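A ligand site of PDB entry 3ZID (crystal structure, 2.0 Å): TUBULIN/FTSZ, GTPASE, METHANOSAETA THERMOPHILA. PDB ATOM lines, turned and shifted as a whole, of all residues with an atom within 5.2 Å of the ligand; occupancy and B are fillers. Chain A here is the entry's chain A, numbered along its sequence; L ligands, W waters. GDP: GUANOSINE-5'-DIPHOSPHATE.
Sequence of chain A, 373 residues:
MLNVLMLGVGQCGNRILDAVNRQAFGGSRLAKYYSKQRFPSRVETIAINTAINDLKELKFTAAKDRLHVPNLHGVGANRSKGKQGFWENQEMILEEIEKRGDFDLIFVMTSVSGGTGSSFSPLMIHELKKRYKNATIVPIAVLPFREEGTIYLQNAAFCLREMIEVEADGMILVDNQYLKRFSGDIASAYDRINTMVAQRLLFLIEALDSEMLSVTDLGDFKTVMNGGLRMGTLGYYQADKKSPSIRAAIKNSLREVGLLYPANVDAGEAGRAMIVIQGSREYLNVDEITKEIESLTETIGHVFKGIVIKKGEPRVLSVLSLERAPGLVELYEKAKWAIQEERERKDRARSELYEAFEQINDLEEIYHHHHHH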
ATOM      1  N   VAL A   9      24.937  -1.734 -23.357  1.00  0.00           N
ATOM      2  CA  VAL A   9      25.468  -1.224 -24.630  1.00  0.00           C
ATOM      3  C   VAL A   9      24.752  -1.855 -25.813  1.00  0.00           C
ATOM      4  O   VAL A   9      24.651  -3.084 -25.921  1.00  0.00           O
ATOM      5  CB  VAL A   9      26.968  -1.524 -24.715  1.00  0.00           C
ATOM      6  CG1 VAL A   9      27.606  -0.873 -25.940  1.00  0.00           C
ATOM      7  CG2 VAL A   9      27.647  -1.055 -23.421  1.00  0.00           C
ATOM      8  N   GLY A  10      24.227  -1.016 -26.701  1.00  0.00           N
ATOM      9  CA  GLY A  10      23.466  -1.530 -27.823  1.00  0.00           C
ATOM     10  C   GLY A  10      22.037  -1.794 -27.400  1.00  0.00           C
ATOM     11  O   GLY A  10      21.701  -1.670 -26.217  1.00  0.00           O
ATOM     12  N   GLN A  11      21.168  -2.156 -28.339  1.00  0.00           N
ATOM     13  CA  GLN A  11      19.754  -2.357 -28.007  1.00  0.00           C
ATOM     14  C   GLN A  11      19.497  -3.413 -26.928  1.00  0.00           C
ATOM     15  O   GLN A  11      18.751  -3.176 -25.960  1.00  0.00           O
ATOM     16  CB  GLN A  11      18.956  -2.713 -29.267  1.00  0.00           C
ATOM     17  CG  GLN A  11      17.534  -3.108 -28.959  1.00  0.00           C
ATOM     18  CD  GLN A  11      16.622  -2.928 -30.137  1.00  0.00           C
ATOM     19  OE1 GLN A  11      15.766  -2.035 -30.153  1.00  0.00           O
ATOM     20  NE2 GLN A  11      16.806  -3.765 -31.146  1.00  0.00           N
ATOM     21  N   CYS A  12      20.104  -4.586 -27.097  1.00  0.00           N
ATOM     22  CA  CYS A  12      19.926  -5.675 -26.146  1.00  0.00           C
ATOM     23  C   CYS A  12      20.444  -5.244 -24.764  1.00  0.00           C
ATOM     24  O   CYS A  12      19.724  -5.348 -23.771  1.00  0.00           O
ATOM     25  CB  CYS A  12      20.628  -6.935 -26.642  1.00  0.00           C
ATOM     26  SG  CYS A  12      20.665  -8.280 -25.460  1.00  0.00           S
ATOM     27  N   GLY A  13      21.677  -4.743 -24.718  1.00  0.00           N
ATOM     28  CA  GLY A  13      22.244  -4.218 -23.497  1.00  0.00           C
ATOM     29  C   GLY A  13      21.365  -3.141 -22.872  1.00  0.00           C
ATOM     30  O   GLY A  13      21.150  -3.150 -21.675  1.00  0.00           O
ATOM     31  N   ARG A  15      18.065  -2.751 -23.165  1.00  0.00           N
ATOM     32  CA  ARG A  15      16.838  -3.332 -22.667  1.00  0.00           C
ATOM     33  C   ARG A  15      17.062  -4.146 -21.398  1.00  0.00           C
ATOM     34  O   ARG A  15      16.219  -4.180 -20.516  1.00  0.00           O
ATOM     35  CB  ARG A  15      16.144  -4.156 -23.744  1.00  0.00           C
ATOM     36  CG  ARG A  15      15.409  -3.339 -24.803  1.00  0.00           C
ATOM     37  CD  ARG A  15      14.956  -4.298 -25.887  1.00  0.00           C
ATOM     38  NE  ARG A  15      14.283  -3.686 -27.018  1.00  0.00           N
ATOM     39  CZ  ARG A  15      14.226  -4.240 -28.218  1.00  0.00           C
ATOM     40  NH1 ARG A  15      14.832  -5.408 -28.431  1.00  0.00           N
ATOM     41  NH2 ARG A  15      13.600  -3.617 -29.204  1.00  0.00           N
ATOM     42  N   ILE A  16      18.215  -4.796 -21.292  1.00  0.00           N
ATOM     43  CA  ILE A  16      18.515  -5.512 -20.065  1.00  0.00           C
ATOM     44  C   ILE A  16      18.733  -4.530 -18.922  1.00  0.00           C
ATOM     45  O   ILE A  16      18.241  -4.733 -17.827  1.00  0.00           O
ATOM     46  CB  ILE A  16      19.743  -6.418 -20.223  1.00  0.00           C
ATOM     47  CG1 ILE A  16      19.386  -7.584 -21.149  1.00  0.00           C
ATOM     48  CG2 ILE A  16      20.181  -6.965 -18.855  1.00  0.00           C
ATOM     49  CD1 ILE A  16      20.603  -8.400 -21.575  1.00  0.00           C
ATOM     50  N   ASN A  49      24.016   3.803 -26.566  1.00  0.00           N
ATOM     51  CA  ASN A  49      23.577   3.395 -27.900  1.00  0.00           C
ATOM     52  C   ASN A  49      23.864   4.439 -28.977  1.00  0.00           C
ATOM     53  O   ASN A  49      23.935   5.634 -28.701  1.00  0.00           O
ATOM     54  CB  ASN A  49      22.068   3.100 -27.890  1.00  0.00           C
ATOM     55  CG  ASN A  49      21.676   2.004 -28.851  1.00  0.00           C
ATOM     56  OD1 ASN A  49      22.232   1.878 -29.952  1.00  0.00           O
ATOM     57  ND2 ASN A  49      20.725   1.168 -28.434  1.00  0.00           N
ATOM     58  N   ASP A  54      16.267   3.626 -29.876  1.00  0.00           N
ATOM     59  CA  ASP A  54      16.407   2.623 -28.832  1.00  0.00           C
ATOM     60  C   ASP A  54      16.389   3.252 -27.446  1.00  0.00           C
ATOM     61  O   ASP A  54      15.735   2.752 -26.544  1.00  0.00           O
ATOM     62  CB  ASP A  54      17.691   1.814 -28.997  1.00  0.00           C
ATOM     63  CG  ASP A  54      17.780   1.099 -30.332  1.00  0.00           C
ATOM     64  OD1 ASP A  54      16.815   1.173 -31.112  1.00  0.00           O
ATOM     65  OD2 ASP A  54      18.830   0.470 -30.592  1.00  0.00           O
ATOM     66  N   GLY A  76      24.291  -0.349 -37.783  1.00  0.00           N
ATOM     67  CA  GLY A  76      23.638  -1.578 -38.150  1.00  0.00           C
ATOM     68  C   GLY A  76      24.293  -2.781 -37.508  1.00  0.00           C
ATOM     69  O   GLY A  76      24.568  -2.776 -36.316  1.00  0.00           O
ATOM     70  N   THR A 110      25.710  -6.576 -23.097  1.00  0.00           N
ATOM     71  CA  THR A 110      25.550  -6.440 -24.529  1.00  0.00           C
ATOM     72  C   THR A 110      25.202  -7.786 -25.162  1.00  0.00           C
ATOM     73  O   THR A 110      25.503  -8.858 -24.598  1.00  0.00           O
ATOM     74  CB  THR A 110      26.864  -5.896 -25.173  1.00  0.00           C
ATOM     75  OG1 THR A 110      26.704  -5.851 -26.589  1.00  0.00           O
ATOM     76  CG2 THR A 110      28.032  -6.833 -24.883  1.00  0.00           C
ATOM     77  N   SER A 111      24.592  -7.750 -26.344  1.00  0.00           N
ATOM     78  CA  SER A 111      24.588  -8.928 -27.213  1.00  0.00           C
ATOM     79  C   SER A 111      25.923  -8.988 -27.951  1.00  0.00           C
ATOM     80  O   SER A 111      26.604  -7.971 -28.121  1.00  0.00           O
ATOM     81  CB  SER A 111      23.437  -8.887 -28.229  1.00  0.00           C
ATOM     82  OG  SER A 111      23.653  -7.911 -29.223  1.00  0.00           O
ATOM     83  N   SER A 113      26.034 -10.176 -31.054  1.00  0.00           N
ATOM     84  CA  SER A 113      25.645 -10.321 -32.469  1.00  0.00           C
ATOM     85  C   SER A 113      25.333  -9.028 -33.226  1.00  0.00           C
ATOM     86  O   SER A 113      25.347  -9.012 -34.455  1.00  0.00           O
ATOM     87  CB  SER A 113      24.456 -11.264 -32.607  1.00  0.00           C
ATOM     88  OG  SER A 113      24.846 -12.607 -32.385  1.00  0.00           O
ATOM     89  N   GLY A 114      25.037  -7.955 -32.515  1.00  0.00           N
ATOM     90  CA  GLY A 114      24.737  -6.718 -33.194  1.00  0.00           C
ATOM     91  C   GLY A 114      26.014  -5.994 -33.612  1.00  0.00           C
ATOM     92  O   GLY A 114      27.117  -6.560 -33.572  1.00  0.00           O
ATOM     93  N   GLY A 115      25.857  -4.748 -34.012  1.00  0.00           N
ATOM     94  CA  GLY A 115      26.989  -3.958 -34.474  1.00  0.00           C
ATOM     95  C   GLY A 115      27.511  -3.025 -33.404  1.00  0.00           C
ATOM     96  O   GLY A 115      28.711  -2.797 -33.301  1.00  0.00           O
ATOM     97  N   THR A 116      26.614  -2.476 -32.588  1.00  0.00           N
ATOM     98  CA  THR A 116      27.028  -1.502 -31.596  1.00  0.00           C
ATOM     99  C   THR A 116      27.551  -2.155 -30.320  1.00  0.00           C
ATOM    100  O   THR A 116      28.715  -1.969 -29.943  1.00  0.00           O
ATOM    101  CB  THR A 116      25.904  -0.494 -31.256  1.00  0.00           C
ATOM    102  OG1 THR A 116      25.627   0.321 -32.394  1.00  0.00           O
ATOM    103  CG2 THR A 116      26.319   0.398 -30.099  1.00  0.00           C
ATOM    104  N   GLY A 117      26.679  -2.914 -29.659  1.00  0.00           N
ATOM    105  CA  GLY A 117      27.076  -3.541 -28.423  1.00  0.00           C
ATOM    106  C   GLY A 117      28.321  -4.399 -28.561  1.00  0.00           C
ATOM    107  O   GLY A 117      29.285  -4.254 -27.808  1.00  0.00           O
ATOM    108  N   SER A 118      28.309  -5.265 -29.562  1.00  0.00           N
ATOM    109  CA  SER A 118      29.343  -6.263 -29.711  1.00  0.00           C
ATOM    110  C   SER A 118      30.712  -5.686 -30.027  1.00  0.00           C
ATOM    111  O   SER A 118      31.711  -6.326 -29.742  1.00  0.00           O
ATOM    112  CB  SER A 118      28.964  -7.267 -30.792  1.00  0.00           C
ATOM    113  OG  SER A 118      29.123  -6.709 -32.081  1.00  0.00           O
ATOM    114  N   VAL A 142      25.153 -11.726 -24.453  1.00  0.00           N
ATOM    115  CA  VAL A 142      23.937 -12.383 -24.920  1.00  0.00           C
ATOM    116  C   VAL A 142      24.119 -13.009 -26.322  1.00  0.00           C
ATOM    117  O   VAL A 142      24.429 -12.301 -27.279  1.00  0.00           O
ATOM    118  CB  VAL A 142      22.754 -11.414 -24.940  1.00  0.00           C
ATOM    119  CG1 VAL A 142      21.536 -12.097 -25.500  1.00  0.00           C
ATOM    120  CG2 VAL A 142      22.505 -10.840 -23.521  1.00  0.00           C
ATOM    121  N   LEU A 143      23.941 -14.321 -26.412  1.00  0.00           N
ATOM    122  CA  LEU A 143      24.150 -15.075 -27.664  1.00  0.00           C
ATOM    123  C   LEU A 143      22.929 -15.070 -28.548  1.00  0.00           C
ATOM    124  O   LEU A 143      21.814 -15.016 -28.030  1.00  0.00           O
ATOM    125  CB  LEU A 143      24.526 -16.531 -27.351  1.00  0.00           C
ATOM    126  CG  LEU A 143      25.619 -16.696 -26.314  1.00  0.00           C
ATOM    127  CD1 LEU A 143      25.842 -18.159 -26.014  1.00  0.00           C
ATOM    128  CD2 LEU A 143      26.886 -16.022 -26.792  1.00  0.00           C
ATOM    129  N   PRO A 144      23.120 -15.191 -29.882  1.00  0.00           N
ATOM    130  CA  PRO A 144      22.006 -15.096 -30.829  1.00  0.00           C
ATOM    131  C   PRO A 144      21.063 -16.289 -30.790  1.00  0.00           C
ATOM    132  O   PRO A 144      21.412 -17.332 -30.245  1.00  0.00           O
ATOM    133  CB  PRO A 144      22.703 -15.020 -32.203  1.00  0.00           C
ATOM    134  CG  PRO A 144      23.988 -15.733 -31.995  1.00  0.00           C
ATOM    135  CD  PRO A 144      24.407 -15.409 -30.567  1.00  0.00           C
ATOM    136  N   PHE A 145      19.850 -16.103 -31.313  1.00  0.00           N
ATOM    137  CA  PHE A 145      18.983 -17.247 -31.644  1.00  0.00           C
ATOM    138  C   PHE A 145      19.675 -18.092 -32.701  1.00  0.00           C
ATOM    139  O   PHE A 145      20.356 -17.557 -33.545  1.00  0.00           O
ATOM    140  CB  PHE A 145      17.654 -16.765 -32.196  1.00  0.00           C
ATOM    141  CG  PHE A 145      16.837 -15.991 -31.227  1.00  0.00           C
ATOM    142  CD1 PHE A 145      16.316 -16.594 -30.096  1.00  0.00           C
ATOM    143  CD2 PHE A 145      16.556 -14.643 -31.463  1.00  0.00           C
ATOM    144  CE1 PHE A 145      15.551 -15.889 -29.204  1.00  0.00           C
ATOM    145  CE2 PHE A 145      15.777 -13.926 -30.578  1.00  0.00           C
ATOM    146  CZ  PHE A 145      15.277 -14.547 -29.437  1.00  0.00           C
ATOM    147  N   GLU A 148      19.021 -17.162 -36.276  1.00  0.00           N
ATOM    148  CA  GLU A 148      19.288 -15.809 -36.700  1.00  0.00           C
ATOM    149  C   GLU A 148      20.298 -15.877 -37.827  1.00  0.00           C
ATOM    150  O   GLU A 148      21.011 -16.866 -37.988  1.00  0.00           O
ATOM    151  CB  GLU A 148      19.756 -14.908 -35.548  1.00  0.00           C
ATOM    152  CG  GLU A 148      18.584 -14.235 -34.843  1.00  0.00           C
ATOM    153  CD  GLU A 148      18.999 -13.384 -33.669  1.00  0.00           C
ATOM    154  OE1 GLU A 148      20.000 -13.715 -32.994  1.00  0.00           O
ATOM    155  OE2 GLU A 148      18.311 -12.360 -33.418  1.00  0.00           O
ATOM    156  N   TYR A 152      24.693 -12.211 -37.886  1.00  0.00           N
ATOM    157  CA  TYR A 152      24.556 -12.361 -36.443  1.00  0.00           C
ATOM    158  C   TYR A 152      25.525 -13.424 -35.914  1.00  0.00           C
ATOM    159  O   TYR A 152      26.228 -13.207 -34.913  1.00  0.00           O
ATOM    160  CB  TYR A 152      23.107 -12.677 -36.093  1.00  0.00           C
ATOM    161  CG  TYR A 152      22.228 -11.443 -36.057  1.00  0.00           C
ATOM    162  CD1 TYR A 152      22.766 -10.169 -36.184  1.00  0.00           C
ATOM    163  CD2 TYR A 152      20.853 -11.550 -35.921  1.00  0.00           C
ATOM    164  CE1 TYR A 152      21.965  -9.032 -36.156  1.00  0.00           C
ATOM    165  CE2 TYR A 152      20.036 -10.427 -35.886  1.00  0.00           C
ATOM    166  CZ  TYR A 152      20.605  -9.165 -36.010  1.00  0.00           C
ATOM    167  OH  TYR A 152      19.798  -8.049 -35.980  1.00  0.00           O
ATOM    168  N   ASN A 176      20.195 -16.819 -25.859  1.00  0.00           N
ATOM    169  CA  ASN A 176      18.842 -16.507 -26.315  1.00  0.00           C
ATOM    170  C   ASN A 176      18.108 -17.748 -26.817  1.00  0.00           C
ATOM    171  O   ASN A 176      16.911 -17.900 -26.608  1.00  0.00           O
ATOM    172  CB  ASN A 176      18.843 -15.442 -27.425  1.00  0.00           C
ATOM    173  CG  ASN A 176      18.778 -14.018 -26.894  1.00  0.00           C
ATOM    174  OD1 ASN A 176      18.704 -13.769 -25.690  1.00  0.00           O
ATOM    175  ND2 ASN A 176      18.820 -13.042 -27.822  1.00  0.00           N
ATOM    176  N   TYR A 190      12.189 -11.611 -25.596  1.00  0.00           N
ATOM    177  CA  TYR A 190      13.150 -10.677 -25.054  1.00  0.00           C
ATOM    178  C   TYR A 190      12.789 -10.297 -23.622  1.00  0.00           C
ATOM    179  O   TYR A 190      13.664 -10.284 -22.771  1.00  0.00           O
ATOM    180  CB  TYR A 190      13.243  -9.397 -25.886  1.00  0.00           C
ATOM    181  CG  TYR A 190      13.927  -9.582 -27.222  1.00  0.00           C
ATOM    182  CD1 TYR A 190      14.808 -10.633 -27.429  1.00  0.00           C
ATOM    183  CD2 TYR A 190      13.737  -8.681 -28.255  1.00  0.00           C
ATOM    184  CE1 TYR A 190      15.444 -10.795 -28.634  1.00  0.00           C
ATOM    185  CE2 TYR A 190      14.389  -8.830 -29.468  1.00  0.00           C
ATOM    186  CZ  TYR A 190      15.237  -9.884 -29.644  1.00  0.00           C
ATOM    187  OH  TYR A 190      15.890 -10.060 -30.852  1.00  0.00           O
ATOM    188  N   ILE A 193      13.578 -13.163 -21.221  1.00  0.00           N
ATOM    189  CA  ILE A 193      15.017 -13.306 -21.042  1.00  0.00           C
ATOM    190  C   ILE A 193      15.585 -12.152 -20.220  1.00  0.00           C
ATOM    191  O   ILE A 193      16.305 -12.389 -19.254  1.00  0.00           O
ATOM    192  CB  ILE A 193      15.739 -13.381 -22.382  1.00  0.00           C
ATOM    193  CG1 ILE A 193      15.365 -14.696 -23.106  1.00  0.00           C
ATOM    194  CG2 ILE A 193      17.243 -13.273 -22.168  1.00  0.00           C
ATOM    195  CD1 ILE A 193      15.712 -14.732 -24.580  1.00  0.00           C
ATOM    196  N   ASN A 194      15.249 -10.920 -20.619  1.00  0.00           N
ATOM    197  CA  ASN A 194      15.774  -9.737 -19.968  1.00  0.00           C
ATOM    198  C   ASN A 194      15.388  -9.724 -18.483  1.00  0.00           C
ATOM    199  O   ASN A 194      16.186  -9.361 -17.623  1.00  0.00           O
ATOM    200  CB  ASN A 194      15.268  -8.443 -20.646  1.00  0.00           C
ATOM    201  CG  ASN A 194      15.719  -8.297 -22.081  1.00  0.00           C
ATOM    202  OD1 ASN A 194      16.535  -9.073 -22.586  1.00  0.00           O
ATOM    203  ND2 ASN A 194      15.157  -7.313 -22.770  1.00  0.00           N
HETATM  204  PB  GDP L   1      23.109  -3.502 -31.560  1.00  0.00           P
HETATM  205  O1B GDP L   1      24.186  -3.806 -30.526  1.00  0.00           O
HETATM  206  O2B GDP L   1      22.165  -2.440 -31.021  1.00  0.00           O
HETATM  207  O3B GDP L   1      23.785  -3.016 -32.829  1.00  0.00           O
HETATM  208  O3A GDP L   1      22.321  -4.856 -31.922  1.00  0.00           O
HETATM  209  PA  GDP L   1      21.442  -5.682 -30.864  1.00  0.00           P
HETATM  210  O1A GDP L   1      19.992  -5.542 -31.165  1.00  0.00           O
HETATM  211  O2A GDP L   1      21.774  -5.355 -29.426  1.00  0.00           O
HETATM  212  O5' GDP L   1      21.982  -7.142 -31.181  1.00  0.00           O
HETATM  213  C5' GDP L   1      21.118  -8.078 -31.805  1.00  0.00           C
HETATM  214  C4' GDP L   1      21.203  -9.376 -31.023  1.00  0.00           C
HETATM  215  O4' GDP L   1      20.673  -9.142 -29.715  1.00  0.00           O
HETATM  216  C3' GDP L   1      20.312 -10.400 -31.685  1.00  0.00           C
HETATM  217  O3' GDP L   1      20.855 -11.672 -31.343  1.00  0.00           O
HETATM  218  C2' GDP L   1      19.005 -10.181 -30.986  1.00  0.00           C
HETATM  219  O2' GDP L   1      18.247 -11.383 -30.996  1.00  0.00           O
HETATM  220  C1' GDP L   1      19.443  -9.844 -29.575  1.00  0.00           C
HETATM  221  N9  GDP L   1      18.561  -8.928 -28.848  1.00  0.00           N
HETATM  222  C8  GDP L   1      18.110  -7.721 -29.254  1.00  0.00           C
HETATM  223  N7  GDP L   1      17.374  -7.136 -28.287  1.00  0.00           N
HETATM  224  C5  GDP L   1      17.343  -7.994 -27.245  1.00  0.00           C
HETATM  225  C6  GDP L   1      16.765  -8.007 -25.890  1.00  0.00           C
HETATM  226  O6  GDP L   1      16.072  -7.059 -25.509  1.00  0.00           O
HETATM  227  N1  GDP L   1      16.979  -9.074 -25.121  1.00  0.00           N
HETATM  228  C2  GDP L   1      17.719 -10.118 -25.533  1.00  0.00           C
HETATM  229  N2  GDP L   1      17.877 -11.152 -24.682  1.00  0.00           N
HETATM  230  N3  GDP L   1      18.294 -10.195 -26.754  1.00  0.00           N
HETATM  231  C4  GDP L   1      18.139  -9.163 -27.614  1.00  0.00           C
HETATM  232  O   HOH W   1      24.071  -0.727 -34.226  1.00  0.00           O
HETATM  233  O   HOH W   2      25.584  -6.061 -30.369  1.00  0.00           O
HETATM  234  O   HOH W   3      22.208   0.325 -31.963  1.00  0.00           O
HETATM  235  O   HOH W   4      20.811  -5.315 -34.335  1.00  0.00           O
HETATM  236  O   HOH W   5      23.465  -5.372 -27.405  1.00  0.00           O
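N1 of the ligand is in hydrogen-bond range of OD1 of Asn 194, 2.6 Å away. OE2 of Glu 148 is in hydrogen-bond range of O2' of the ligand (2.6 Å). An oxygen (O5') of the ligand sits at hydrogen-bond distance from the side-chain hydroxyl (OG) of Ser 111, 2.7 Å away. An oxygen (O2') of the ligand is in hydrogen-bond range of the side-chain hydroxyl (OH) of Tyr 190. An oxygen (O1B) of the ligand lies within hydrogen-bond range of the backbone NH (N) of Gly 117 (2.8 Å). The backbone NH of Gln 11 sits at hydrogen-bond distance from an oxygen (O2B) of the ligand (2.9 Å). The backbone NH (N) of Thr 116 sits at hydrogen-bond distance from an oxygen (O3B) of the ligand (2.9 Å). The side-chain amide oxygen of Asn 176 sits at hydrogen-bond distance from a nitrogen (N2) of the ligand. The backbone NH (N) of Gly 115 is in hydrogen-bond range of an oxygen (O3B) of the ligand (2.9 Å). N of Cys 12 lies within hydrogen-bond range of O2A of the ligand, 3.0 Å away. SG of Cys 12 sits at hydrogen-bond distance from N3 of the ligand, at 3.3 Å. A nitrogen (N7) of the ligand sits at hydrogen-bond distance from the guanidinium group (NH1) of Arg 15, at 3.1 Å. The backbone NH of Gly 114 lies within hydrogen-bond range of an oxygen (O5') of the ligand.
O of Tyr 190 sits close to OD1 of Asn 194 (3.1 Å). The side-chain carboxylate (OE1) of Glu 148 is in hydrogen-bond range of the backbone NH (N) of Phe 145, 2.9 Å away. The backbone carbonyl oxygen (O) of Gly 117 lies close to the side-chain hydroxyl (OG1) of Thr 110 (3.3 Å). The guanidinium group of Arg 15 is in hydrogen-bond range of the side-chain amide oxygen of Gln 11 (2.8 Å). The backbone NH of Asn 176 sits close to the backbone carbonyl oxygen of Leu 143, at 3.3 Å. N of Gly 115 sits close to O of Gly 76. OG of Ser 113 is in hydrogen-bond range of O of Tyr 152. The backbone NH (N) of Val 142 sits at hydrogen-bond distance from the backbone carbonyl oxygen (O) of Thr 110, at 2.9 Å.
Gly 10 touches the ligand. Gly 76 touches the ligand. Ser 113 touches the ligand. CG1 of Val 142 touches N2 of the ligand (3.9 Å). CA of Pro 144 touches O3' of the ligand, 3.6 Å away. Phe 145 touches the ligand (CE2 to O2', 3.6 Å). Ile 193 touches the ligand. Along chain A the residues within 4 Å of the ligand span positions 10 to 194.
Water W1 lies within hydrogen-bond range of the side-chain hydroxyl of Thr 116, an oxygen (O3B) of the ligand and the backbone carbonyl oxygen of Gly 76. Water W4 lies within hydrogen-bond range of an oxygen (O3A) of the ligand (2.9 Å) and the side-chain hydroxyl (OH) of Tyr 152 (3.3 Å). Water W3 lies within hydrogen-bond range of the side-chain amide oxygen of Asn 49, an oxygen (O2B) of the ligand and the side-chain hydroxyl of Thr 116.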
